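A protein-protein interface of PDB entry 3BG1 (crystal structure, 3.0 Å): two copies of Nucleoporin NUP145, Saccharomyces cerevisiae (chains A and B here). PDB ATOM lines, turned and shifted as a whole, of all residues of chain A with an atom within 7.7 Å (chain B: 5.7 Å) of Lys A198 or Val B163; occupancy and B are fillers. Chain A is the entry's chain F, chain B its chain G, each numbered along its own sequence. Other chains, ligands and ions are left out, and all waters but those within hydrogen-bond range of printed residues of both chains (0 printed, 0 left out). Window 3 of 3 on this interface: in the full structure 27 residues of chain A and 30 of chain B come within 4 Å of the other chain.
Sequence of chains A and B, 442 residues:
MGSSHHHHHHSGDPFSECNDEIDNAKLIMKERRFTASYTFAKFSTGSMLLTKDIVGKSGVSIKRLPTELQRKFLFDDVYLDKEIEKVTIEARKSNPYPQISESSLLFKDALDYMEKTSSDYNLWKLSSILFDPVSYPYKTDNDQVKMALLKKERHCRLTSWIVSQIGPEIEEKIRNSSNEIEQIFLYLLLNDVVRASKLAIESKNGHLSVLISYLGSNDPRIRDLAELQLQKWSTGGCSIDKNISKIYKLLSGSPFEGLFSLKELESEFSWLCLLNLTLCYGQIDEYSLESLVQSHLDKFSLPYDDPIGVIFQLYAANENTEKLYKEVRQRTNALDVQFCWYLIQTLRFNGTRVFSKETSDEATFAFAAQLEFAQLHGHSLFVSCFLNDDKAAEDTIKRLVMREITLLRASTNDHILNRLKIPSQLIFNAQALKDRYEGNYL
The guanidinium group (NE) of Arg B195 lies within salt-bridge range of the side-chain carboxylate (OD2) of Asp B192 (2.8 Å).
Among the printed residues, pairs that only touch across the chains: Val A194 with Asn B191 (3.2 Å), Val A194 with Asp B192 (3.7 Å), Lys A198 with Val B163 (3.8 Å) and Ile A201 with Ser B160 (3.1 Å).
Of chain A, only Lys A198 comes within 4 Å of Val B163. Printed residues of chain A within 4 Å of Ser B160: Ile A201. Of the printed residues of chain A, Asn B191 touches Val A194. Of the printed residues of chain B, Ile A201 touches Ser B160 (3.1 Å). Asp A192 touches none of the printed residues of chain B. Ile B162 touches none of the printed residues of chain A. The nearest residue of chain A that does not touch Val B163 is Val A194 (6.4 Å).
Of the 16 printed residues of chain B, 4 touch a printed residue of chain A. Printed residues of chain B that touch a printed residue of chain A: Ser B160, Val B163, Asn B191 and Asp B192. Hydrophobic or aromatic side chains of chain B within 4 Å of the printed part of chain A: Val B163. Along chain A the printed residues that touch a printed residue of chain B span positions 194 to 201. Among the printed residues, 4 pairs touch across the chains.
2 positions are printed for both chains.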
ATOM      1  N   ILE A 184       0.483 -11.253 -20.426  1.00  0.00           N
ATOM      2  CA  ILE A 184       1.621 -10.434 -20.823  1.00  0.00           C
ATOM      3  C   ILE A 184       1.552 -10.062 -22.293  1.00  0.00           C
ATOM      4  O   ILE A 184       1.587  -8.883 -22.651  1.00  0.00           O
ATOM      5  CB  ILE A 184       2.963 -11.131 -20.583  1.00  0.00           C
ATOM      6  CG1 ILE A 184       3.047 -11.620 -19.135  1.00  0.00           C
ATOM      7  CG2 ILE A 184       4.099 -10.142 -20.896  1.00  0.00           C
ATOM      8  CD1 ILE A 184       4.454 -11.948 -18.654  1.00  0.00           C
ATOM      9  N   TYR A 187      -0.532  -7.167 -22.812  1.00  0.00           N
ATOM     10  CA  TYR A 187      -0.042  -5.855 -22.418  1.00  0.00           C
ATOM     11  C   TYR A 187       0.898  -5.309 -23.475  1.00  0.00           C
ATOM     12  O   TYR A 187       1.000  -4.098 -23.678  1.00  0.00           O
ATOM     13  CB  TYR A 187       0.647  -5.923 -21.054  1.00  0.00           C
ATOM     14  CG  TYR A 187      -0.302  -5.668 -19.895  1.00  0.00           C
ATOM     15  CD1 TYR A 187      -1.456  -6.437 -19.726  1.00  0.00           C
ATOM     16  CD2 TYR A 187      -0.055  -4.645 -18.977  1.00  0.00           C
ATOM     17  CE1 TYR A 187      -2.340  -6.191 -18.674  1.00  0.00           C
ATOM     18  CE2 TYR A 187      -0.935  -4.392 -17.924  1.00  0.00           C
ATOM     19  CZ  TYR A 187      -2.074  -5.169 -17.781  1.00  0.00           C
ATOM     20  OH  TYR A 187      -2.944  -4.924 -16.744  1.00  0.00           O
ATOM     21  N   ASP A 192       2.292  -1.535 -23.912  1.00  0.00           N
ATOM     22  CA  ASP A 192       2.634  -1.201 -22.536  1.00  0.00           C
ATOM     23  C   ASP A 192       3.669  -2.203 -22.036  1.00  0.00           C
ATOM     24  O   ASP A 192       3.338  -3.297 -21.561  1.00  0.00           O
ATOM     25  CB  ASP A 192       1.421  -1.194 -21.600  1.00  0.00           C
ATOM     26  CG  ASP A 192       1.804  -0.825 -20.159  1.00  0.00           C
ATOM     27  OD1 ASP A 192       2.555  -1.602 -19.522  1.00  0.00           O
ATOM     28  OD2 ASP A 192       1.366   0.243 -19.667  1.00  0.00           O
ATOM     29  N   VAL A 193       4.931  -1.810 -22.161  1.00  0.00           N
ATOM     30  CA  VAL A 193       6.037  -2.644 -21.749  1.00  0.00           C
ATOM     31  C   VAL A 193       6.196  -2.649 -20.246  1.00  0.00           C
ATOM     32  O   VAL A 193       6.377  -3.709 -19.641  1.00  0.00           O
ATOM     33  CB  VAL A 193       7.345  -2.152 -22.374  1.00  0.00           C
ATOM     34  CG1 VAL A 193       8.541  -2.751 -21.644  1.00  0.00           C
ATOM     35  CG2 VAL A 193       7.380  -2.535 -23.828  1.00  0.00           C
ATOM     36  N   VAL A 194       6.133  -1.465 -19.642  1.00  0.00           N
ATOM     37  CA  VAL A 194       6.302  -1.370 -18.199  1.00  0.00           C
ATOM     38  C   VAL A 194       5.442  -2.374 -17.437  1.00  0.00           C
ATOM     39  O   VAL A 194       5.954  -3.148 -16.619  1.00  0.00           O
ATOM     40  CB  VAL A 194       5.993   0.044 -17.670  1.00  0.00           C
ATOM     41  CG1 VAL A 194       6.051   0.045 -16.154  1.00  0.00           C
ATOM     42  CG2 VAL A 194       7.010   1.034 -18.203  1.00  0.00           C
ATOM     43  N   ARG A 195       4.140  -2.374 -17.701  1.00  0.00           N
ATOM     44  CA  ARG A 195       3.280  -3.301 -16.998  1.00  0.00           C
ATOM     45  C   ARG A 195       3.453  -4.738 -17.521  1.00  0.00           C
ATOM     46  O   ARG A 195       3.383  -5.703 -16.755  1.00  0.00           O
ATOM     47  CB  ARG A 195       1.828  -2.805 -17.051  1.00  0.00           C
ATOM     48  CG  ARG A 195       1.610  -1.530 -16.211  1.00  0.00           C
ATOM     49  CD  ARG A 195       0.134  -1.173 -16.028  1.00  0.00           C
ATOM     50  NE  ARG A 195      -0.426  -0.426 -17.157  1.00  0.00           N
ATOM     51  CZ  ARG A 195      -1.719  -0.127 -17.303  1.00  0.00           C
ATOM     52  NH1 ARG A 195      -2.604  -0.512 -16.392  1.00  0.00           N
ATOM     53  NH2 ARG A 195      -2.129   0.564 -18.363  1.00  0.00           N
ATOM     54  N   ALA A 196       3.735  -4.889 -18.812  1.00  0.00           N
ATOM     55  CA  ALA A 196       3.938  -6.227 -19.384  1.00  0.00           C
ATOM     56  C   ALA A 196       5.127  -6.908 -18.711  1.00  0.00           C
ATOM     57  O   ALA A 196       5.129  -8.120 -18.501  1.00  0.00           O
ATOM     58  CB  ALA A 196       4.176  -6.129 -20.892  1.00  0.00           C
ATOM     59  N   SER A 197       6.134  -6.103 -18.388  1.00  0.00           N
ATOM     60  CA  SER A 197       7.343  -6.575 -17.727  1.00  0.00           C
ATOM     61  C   SER A 197       7.042  -6.941 -16.270  1.00  0.00           C
ATOM     62  O   SER A 197       7.306  -8.071 -15.837  1.00  0.00           O
ATOM     63  CB  SER A 197       8.425  -5.484 -17.779  1.00  0.00           C
ATOM     64  OG  SER A 197       9.526  -5.788 -16.934  1.00  0.00           O
ATOM     65  N   LYS A 198       6.496  -5.983 -15.520  1.00  0.00           N
ATOM     66  CA  LYS A 198       6.152  -6.206 -14.120  1.00  0.00           C
ATOM     67  C   LYS A 198       5.490  -7.569 -13.996  1.00  0.00           C
ATOM     68  O   LYS A 198       5.927  -8.411 -13.215  1.00  0.00           O
ATOM     69  CB  LYS A 198       5.204  -5.109 -13.603  1.00  0.00           C
ATOM     70  CG  LYS A 198       5.907  -3.801 -13.188  1.00  0.00           C
ATOM     71  CD  LYS A 198       4.960  -2.734 -12.586  1.00  0.00           C
ATOM     72  CE  LYS A 198       5.743  -1.481 -12.147  1.00  0.00           C
ATOM     73  NZ  LYS A 198       4.885  -0.325 -11.756  1.00  0.00           N
ATOM     74  N   LEU A 199       4.448  -7.797 -14.786  1.00  0.00           N
ATOM     75  CA  LEU A 199       3.757  -9.075 -14.741  1.00  0.00           C
ATOM     76  C   LEU A 199       4.714 -10.249 -14.931  1.00  0.00           C
ATOM     77  O   LEU A 199       4.652 -11.233 -14.196  1.00  0.00           O
ATOM     78  CB  LEU A 199       2.683  -9.150 -15.822  1.00  0.00           C
ATOM     79  CG  LEU A 199       1.710 -10.303 -15.552  1.00  0.00           C
ATOM     80  CD1 LEU A 199       0.902  -9.905 -14.317  1.00  0.00           C
ATOM     81  CD2 LEU A 199       0.779 -10.587 -16.734  1.00  0.00           C
ATOM     82  N   ALA A 200       5.593 -10.143 -15.920  1.00  0.00           N
ATOM     83  CA  ALA A 200       6.546 -11.206 -16.213  1.00  0.00           C
ATOM     84  C   ALA A 200       7.360 -11.642 -14.994  1.00  0.00           C
ATOM     85  O   ALA A 200       7.489 -12.835 -14.708  1.00  0.00           O
ATOM     86  CB  ALA A 200       7.478 -10.763 -17.334  1.00  0.00           C
ATOM     87  N   ILE A 201       7.915 -10.677 -14.279  1.00  0.00           N
ATOM     88  CA  ILE A 201       8.705 -10.996 -13.108  1.00  0.00           C
ATOM     89  C   ILE A 201       7.822 -11.563 -12.025  1.00  0.00           C
ATOM     90  O   ILE A 201       8.156 -12.578 -11.426  1.00  0.00           O
ATOM     91  CB  ILE A 201       9.380  -9.758 -12.533  1.00  0.00           C
ATOM     92  CG1 ILE A 201      10.340  -9.180 -13.560  1.00  0.00           C
ATOM     93  CG2 ILE A 201      10.103 -10.104 -11.246  1.00  0.00           C
ATOM     94  CD1 ILE A 201      10.770  -7.771 -13.236  1.00  0.00           C
ATOM     95  N   GLU A 202       6.694 -10.910 -11.778  1.00  0.00           N
ATOM     96  CA  GLU A 202       5.791 -11.346 -10.723  1.00  0.00           C
ATOM     97  C   GLU A 202       5.169 -12.729 -10.890  1.00  0.00           C
ATOM     98  O   GLU A 202       4.570 -13.259  -9.954  1.00  0.00           O
ATOM     99  CB  GLU A 202       4.683 -10.315 -10.511  1.00  0.00           C
ATOM    100  CG  GLU A 202       3.677 -10.733  -9.446  1.00  0.00           C
ATOM    101  CD  GLU A 202       2.824  -9.586  -8.952  1.00  0.00           C
ATOM    102  OE1 GLU A 202       2.774  -8.545  -9.645  1.00  0.00           O
ATOM    103  OE2 GLU A 202       2.199  -9.733  -7.876  1.00  0.00           O
ATOM    104  N   SER A 203       5.310 -13.329 -12.062  1.00  0.00           N
ATOM    105  CA  SER A 203       4.737 -14.650 -12.266  1.00  0.00           C
ATOM    106  C   SER A 203       5.820 -15.718 -12.304  1.00  0.00           C
ATOM    107  O   SER A 203       5.537 -16.880 -12.599  1.00  0.00           O
ATOM    108  CB  SER A 203       3.987 -14.694 -13.579  1.00  0.00           C
ATOM    109  OG  SER A 203       4.921 -14.642 -14.644  1.00  0.00           O
ATOM    110  N   LYS A 204       7.058 -15.324 -12.020  1.00  0.00           N
ATOM    111  CA  LYS A 204       8.183 -16.254 -12.042  1.00  0.00           C
ATOM    112  C   LYS A 204       8.414 -16.675 -13.501  1.00  0.00           C
ATOM    113  O   LYS A 204       8.607 -17.855 -13.812  1.00  0.00           O
ATOM    114  CB  LYS A 204       7.882 -17.481 -11.163  1.00  0.00           C
ATOM    115  CG  LYS A 204       9.105 -18.308 -10.733  1.00  0.00           C
ATOM    116  CD  LYS A 204       9.741 -17.796  -9.434  1.00  0.00           C
ATOM    117  CE  LYS A 204      10.888 -18.701  -8.976  1.00  0.00           C
ATOM    118  NZ  LYS A 204      11.486 -18.268  -7.683  1.00  0.00           N
ATOM    119  N   SER A 209      10.924 -10.751 -19.129  1.00  0.00           N
ATOM    120  CA  SER A 209      11.130  -9.370 -18.750  1.00  0.00           C
ATOM    121  C   SER A 209      12.414  -8.864 -19.390  1.00  0.00           C
ATOM    122  O   SER A 209      12.585  -7.660 -19.599  1.00  0.00           O
ATOM    123  CB  SER A 209      11.218  -9.247 -17.233  1.00  0.00           C
ATOM    124  OG  SER A 209      11.023  -7.902 -16.832  1.00  0.00           O
ATOM    125  N   ILE A 212      11.563  -8.576 -23.356  1.00  0.00           N
ATOM    126  CA  ILE A 212      10.671  -7.423 -23.366  1.00  0.00           C
ATOM    127  C   ILE A 212      11.500  -6.143 -23.274  1.00  0.00           C
ATOM    128  O   ILE A 212      11.143  -5.117 -23.849  1.00  0.00           O
ATOM    129  CB  ILE A 212       9.700  -7.474 -22.172  1.00  0.00           C
ATOM    130  CG1 ILE A 212       8.564  -8.434 -22.485  1.00  0.00           C
ATOM    131  CG2 ILE A 212       9.166  -6.090 -21.860  1.00  0.00           C
ATOM    132  CD1 ILE A 212       7.527  -8.510 -21.402  1.00  0.00           C
ATOM    133  N   LEU B 158      16.644  -6.070 -10.601  1.00  0.00           N
ATOM    134  CA  LEU B 158      16.916  -5.126  -9.546  1.00  0.00           C
ATOM    135  C   LEU B 158      16.144  -3.821  -9.685  1.00  0.00           C
ATOM    136  O   LEU B 158      15.506  -3.379  -8.733  1.00  0.00           O
ATOM    137  CB  LEU B 158      18.401  -4.823  -9.447  1.00  0.00           C
ATOM    138  CG  LEU B 158      18.604  -3.721  -8.400  1.00  0.00           C
ATOM    139  CD1 LEU B 158      19.744  -4.071  -7.487  1.00  0.00           C
ATOM    140  CD2 LEU B 158      18.862  -2.383  -9.066  1.00  0.00           C
ATOM    141  N   THR B 159      16.200  -3.173 -10.840  1.00  0.00           N
ATOM    142  CA  THR B 159      15.458  -1.928 -10.951  1.00  0.00           C
ATOM    143  C   THR B 159      13.993  -2.234 -10.676  1.00  0.00           C
ATOM    144  O   THR B 159      13.340  -1.526  -9.912  1.00  0.00           O
ATOM    145  CB  THR B 159      15.600  -1.288 -12.340  1.00  0.00           C
ATOM    146  OG1 THR B 159      15.032  -2.150 -13.335  1.00  0.00           O
ATOM    147  CG2 THR B 159      17.057  -1.043 -12.647  1.00  0.00           C
ATOM    148  N   SER B 160      13.491  -3.310 -11.278  1.00  0.00           N
ATOM    149  CA  SER B 160      12.100  -3.708 -11.095  1.00  0.00           C
ATOM    150  C   SER B 160      11.721  -3.789  -9.624  1.00  0.00           C
ATOM    151  O   SER B 160      10.573  -3.569  -9.259  1.00  0.00           O
ATOM    152  CB  SER B 160      11.842  -5.045 -11.781  1.00  0.00           C
ATOM    153  OG  SER B 160      11.917  -4.894 -13.190  1.00  0.00           O
ATOM    154  N   TRP B 161      12.697  -4.102  -8.785  1.00  0.00           N
ATOM    155  CA  TRP B 161      12.484  -4.181  -7.345  1.00  0.00           C
ATOM    156  C   TRP B 161      12.343  -2.771  -6.784  1.00  0.00           C
ATOM    157  O   TRP B 161      11.311  -2.418  -6.221  1.00  0.00           O
ATOM    158  CB  TRP B 161      13.682  -4.852  -6.692  1.00  0.00           C
ATOM    159  CG  TRP B 161      13.680  -4.875  -5.199  1.00  0.00           C
ATOM    160  CD1 TRP B 161      13.042  -5.779  -4.401  1.00  0.00           C
ATOM    161  CD2 TRP B 161      14.481  -4.063  -4.325  1.00  0.00           C
ATOM    162  NE1 TRP B 161      13.412  -5.597  -3.088  1.00  0.00           N
ATOM    163  CE2 TRP B 161      14.294  -4.550  -3.014  1.00  0.00           C
ATOM    164  CE3 TRP B 161      15.341  -2.976  -4.524  1.00  0.00           C
ATOM    165  CZ2 TRP B 161      14.944  -3.998  -1.905  1.00  0.00           C
ATOM    166  CZ3 TRP B 161      15.991  -2.421  -3.413  1.00  0.00           C
ATOM    167  CH2 TRP B 161      15.787  -2.936  -2.124  1.00  0.00           C
ATOM    168  N   ILE B 162      13.391  -1.970  -6.935  1.00  0.00           N
ATOM    169  CA  ILE B 162      13.366  -0.603  -6.439  1.00  0.00           C
ATOM    170  C   ILE B 162      12.101   0.129  -6.894  1.00  0.00           C
ATOM    171  O   ILE B 162      11.620   1.033  -6.207  1.00  0.00           O
ATOM    172  CB  ILE B 162      14.574   0.184  -6.933  1.00  0.00           C
ATOM    173  CG1 ILE B 162      15.803  -0.710  -6.922  1.00  0.00           C
ATOM    174  CG2 ILE B 162      14.816   1.380  -6.032  1.00  0.00           C
ATOM    175  CD1 ILE B 162      17.032  -0.010  -7.436  1.00  0.00           C
ATOM    176  N   VAL B 163      11.567  -0.254  -8.051  1.00  0.00           N
ATOM    177  CA  VAL B 163      10.355   0.384  -8.553  1.00  0.00           C
ATOM    178  C   VAL B 163       9.249   0.132  -7.547  1.00  0.00           C
ATOM    179  O   VAL B 163       8.412   0.996  -7.310  1.00  0.00           O
ATOM    180  CB  VAL B 163       9.921  -0.175  -9.933  1.00  0.00           C
ATOM    181  CG1 VAL B 163       8.561   0.394 -10.328  1.00  0.00           C
ATOM    182  CG2 VAL B 163      10.949   0.196 -10.988  1.00  0.00           C
ATOM    183  N   SER B 164       9.256  -1.051  -6.944  1.00  0.00           N
ATOM    184  CA  SER B 164       8.245  -1.389  -5.953  1.00  0.00           C
ATOM    185  C   SER B 164       8.526  -0.749  -4.604  1.00  0.00           C
ATOM    186  O   SER B 164       7.603  -0.507  -3.829  1.00  0.00           O
ATOM    187  CB  SER B 164       8.144  -2.900  -5.792  1.00  0.00           C
ATOM    188  OG  SER B 164       7.654  -3.478  -6.986  1.00  0.00           O
ATOM    189  N   GLN B 165       9.792  -0.468  -4.325  1.00  0.00           N
ATOM    190  CA  GLN B 165      10.168   0.156  -3.064  1.00  0.00           C
ATOM    191  C   GLN B 165       9.896   1.662  -3.094  1.00  0.00           C
ATOM    192  O   GLN B 165       9.700   2.306  -2.063  1.00  0.00           O
ATOM    193  CB  GLN B 165      11.649  -0.091  -2.791  1.00  0.00           C
ATOM    194  CG  GLN B 165      12.042  -1.556  -2.789  1.00  0.00           C
ATOM    195  CD  GLN B 165      11.492  -2.317  -1.598  1.00  0.00           C
ATOM    196  OE1 GLN B 165      11.813  -2.012  -0.441  1.00  0.00           O
ATOM    197  NE2 GLN B 165      10.662  -3.319  -1.873  1.00  0.00           N
ATOM    198  N   ILE B 166       9.872   2.230  -4.285  1.00  0.00           N
ATOM    199  CA  ILE B 166       9.638   3.656  -4.412  1.00  0.00           C
ATOM    200  C   ILE B 166       8.228   3.913  -4.936  1.00  0.00           C
ATOM    201  O   ILE B 166       7.820   5.054  -5.164  1.00  0.00           O
ATOM    202  CB  ILE B 166      10.720   4.243  -5.325  1.00  0.00           C
ATOM    203  CG1 ILE B 166      12.074   4.014  -4.653  1.00  0.00           C
ATOM    204  CG2 ILE B 166      10.498   5.714  -5.563  1.00  0.00           C
ATOM    205  CD1 ILE B 166      13.229   4.445  -5.467  1.00  0.00           C
ATOM    206  N   GLY B 167       7.478   2.826  -5.095  1.00  0.00           N
ATOM    207  CA  GLY B 167       6.114   2.923  -5.577  1.00  0.00           C
ATOM    208  C   GLY B 167       5.286   3.837  -4.698  1.00  0.00           C
ATOM    209  O   GLY B 167       4.826   4.883  -5.149  1.00  0.00           O
ATOM    210  N   PRO B 168       5.079   3.472  -3.429  1.00  0.00           N
ATOM    211  CA  PRO B 168       4.281   4.377  -2.604  1.00  0.00           C
ATOM    212  C   PRO B 168       4.858   5.792  -2.631  1.00  0.00           C
ATOM    213  O   PRO B 168       4.152   6.758  -2.917  1.00  0.00           O
ATOM    214  CB  PRO B 168       4.371   3.737  -1.221  1.00  0.00           C
ATOM    215  CG  PRO B 168       5.725   3.076  -1.238  1.00  0.00           C
ATOM    216  CD  PRO B 168       5.728   2.437  -2.602  1.00  0.00           C
ATOM    217  N   LEU B 190       9.737   6.275 -12.007  1.00  0.00           N
ATOM    218  CA  LEU B 190       9.271   4.954 -11.624  1.00  0.00           C
ATOM    219  C   LEU B 190       9.494   3.991 -12.769  1.00  0.00           C
ATOM    220  O   LEU B 190       8.920   2.895 -12.798  1.00  0.00           O
ATOM    221  CB  LEU B 190       7.797   4.982 -11.237  1.00  0.00           C
ATOM    222  CG  LEU B 190       7.477   5.961 -10.111  1.00  0.00           C
ATOM    223  CD1 LEU B 190       6.079   5.671  -9.613  1.00  0.00           C
ATOM    224  CD2 LEU B 190       8.479   5.816  -8.978  1.00  0.00           C
ATOM    225  N   ASN B 191      10.364   4.385 -13.702  1.00  0.00           N
ATOM    226  CA  ASN B 191      10.678   3.532 -14.838  1.00  0.00           C
ATOM    227  C   ASN B 191       9.344   3.219 -15.539  1.00  0.00           C
ATOM    228  O   ASN B 191       9.134   2.123 -16.095  1.00  0.00           O
ATOM    229  CB  ASN B 191      11.334   2.248 -14.315  1.00  0.00           C
ATOM    230  CG  ASN B 191      11.897   1.380 -15.415  1.00  0.00           C
ATOM    231  OD1 ASN B 191      12.767   1.812 -16.167  1.00  0.00           O
ATOM    232  ND2 ASN B 191      11.412   0.140 -15.507  1.00  0.00           N
ATOM    233  N   ASP B 192       8.436   4.191 -15.492  1.00  0.00           N
ATOM    234  CA  ASP B 192       7.118   4.051 -16.107  1.00  0.00           C
ATOM    235  C   ASP B 192       7.024   4.972 -17.330  1.00  0.00           C
ATOM    236  O   ASP B 192       6.385   6.034 -17.295  1.00  0.00           O
ATOM    237  CB  ASP B 192       6.031   4.405 -15.095  1.00  0.00           C
ATOM    238  CG  ASP B 192       4.654   3.995 -15.555  1.00  0.00           C
ATOM    239  OD1 ASP B 192       4.328   4.255 -16.734  1.00  0.00           O
ATOM    240  OD2 ASP B 192       3.901   3.418 -14.738  1.00  0.00           O
ATOM    241  N   ARG B 195       3.249   5.362 -19.167  1.00  0.00           N
ATOM    242  CA  ARG B 195       2.370   6.383 -18.639  1.00  0.00           C
ATOM    243  C   ARG B 195       3.017   7.775 -18.711  1.00  0.00           C
ATOM    244  O   ARG B 195       2.334   8.775 -18.952  1.00  0.00           O
ATOM    245  CB  ARG B 195       1.918   5.995 -17.227  1.00  0.00           C
ATOM    246  CG  ARG B 195       0.968   4.780 -17.225  1.00  0.00           C
ATOM    247  CD  ARG B 195       0.291   4.543 -15.873  1.00  0.00           C
ATOM    248  NE  ARG B 195       1.125   3.792 -14.929  1.00  0.00           N
ATOM    249  CZ  ARG B 195       0.823   3.587 -13.646  1.00  0.00           C
ATOM    250  NH1 ARG B 195      -0.300   4.079 -13.134  1.00  0.00           N
ATOM    251  NH2 ARG B 195       1.642   2.883 -12.871  1.00  0.00           N
ATOM    252  N   ASN B 276      17.975   4.517  -8.211  1.00  0.00           N
ATOM    253  CA  ASN B 276      17.256   3.957  -9.337  1.00  0.00           C
ATOM    254  C   ASN B 276      17.527   4.755 -10.594  1.00  0.00           C
ATOM    255  O   ASN B 276      17.504   4.208 -11.693  1.00  0.00           O
ATOM    256  CB  ASN B 276      15.758   3.915  -9.105  1.00  0.00           C
ATOM    257  CG  ASN B 276      15.046   3.136 -10.191  1.00  0.00           C
ATOM    258  OD1 ASN B 276      15.249   1.928 -10.334  1.00  0.00           O
ATOM    259  ND2 ASN B 276      14.225   3.821 -10.973  1.00  0.00           N
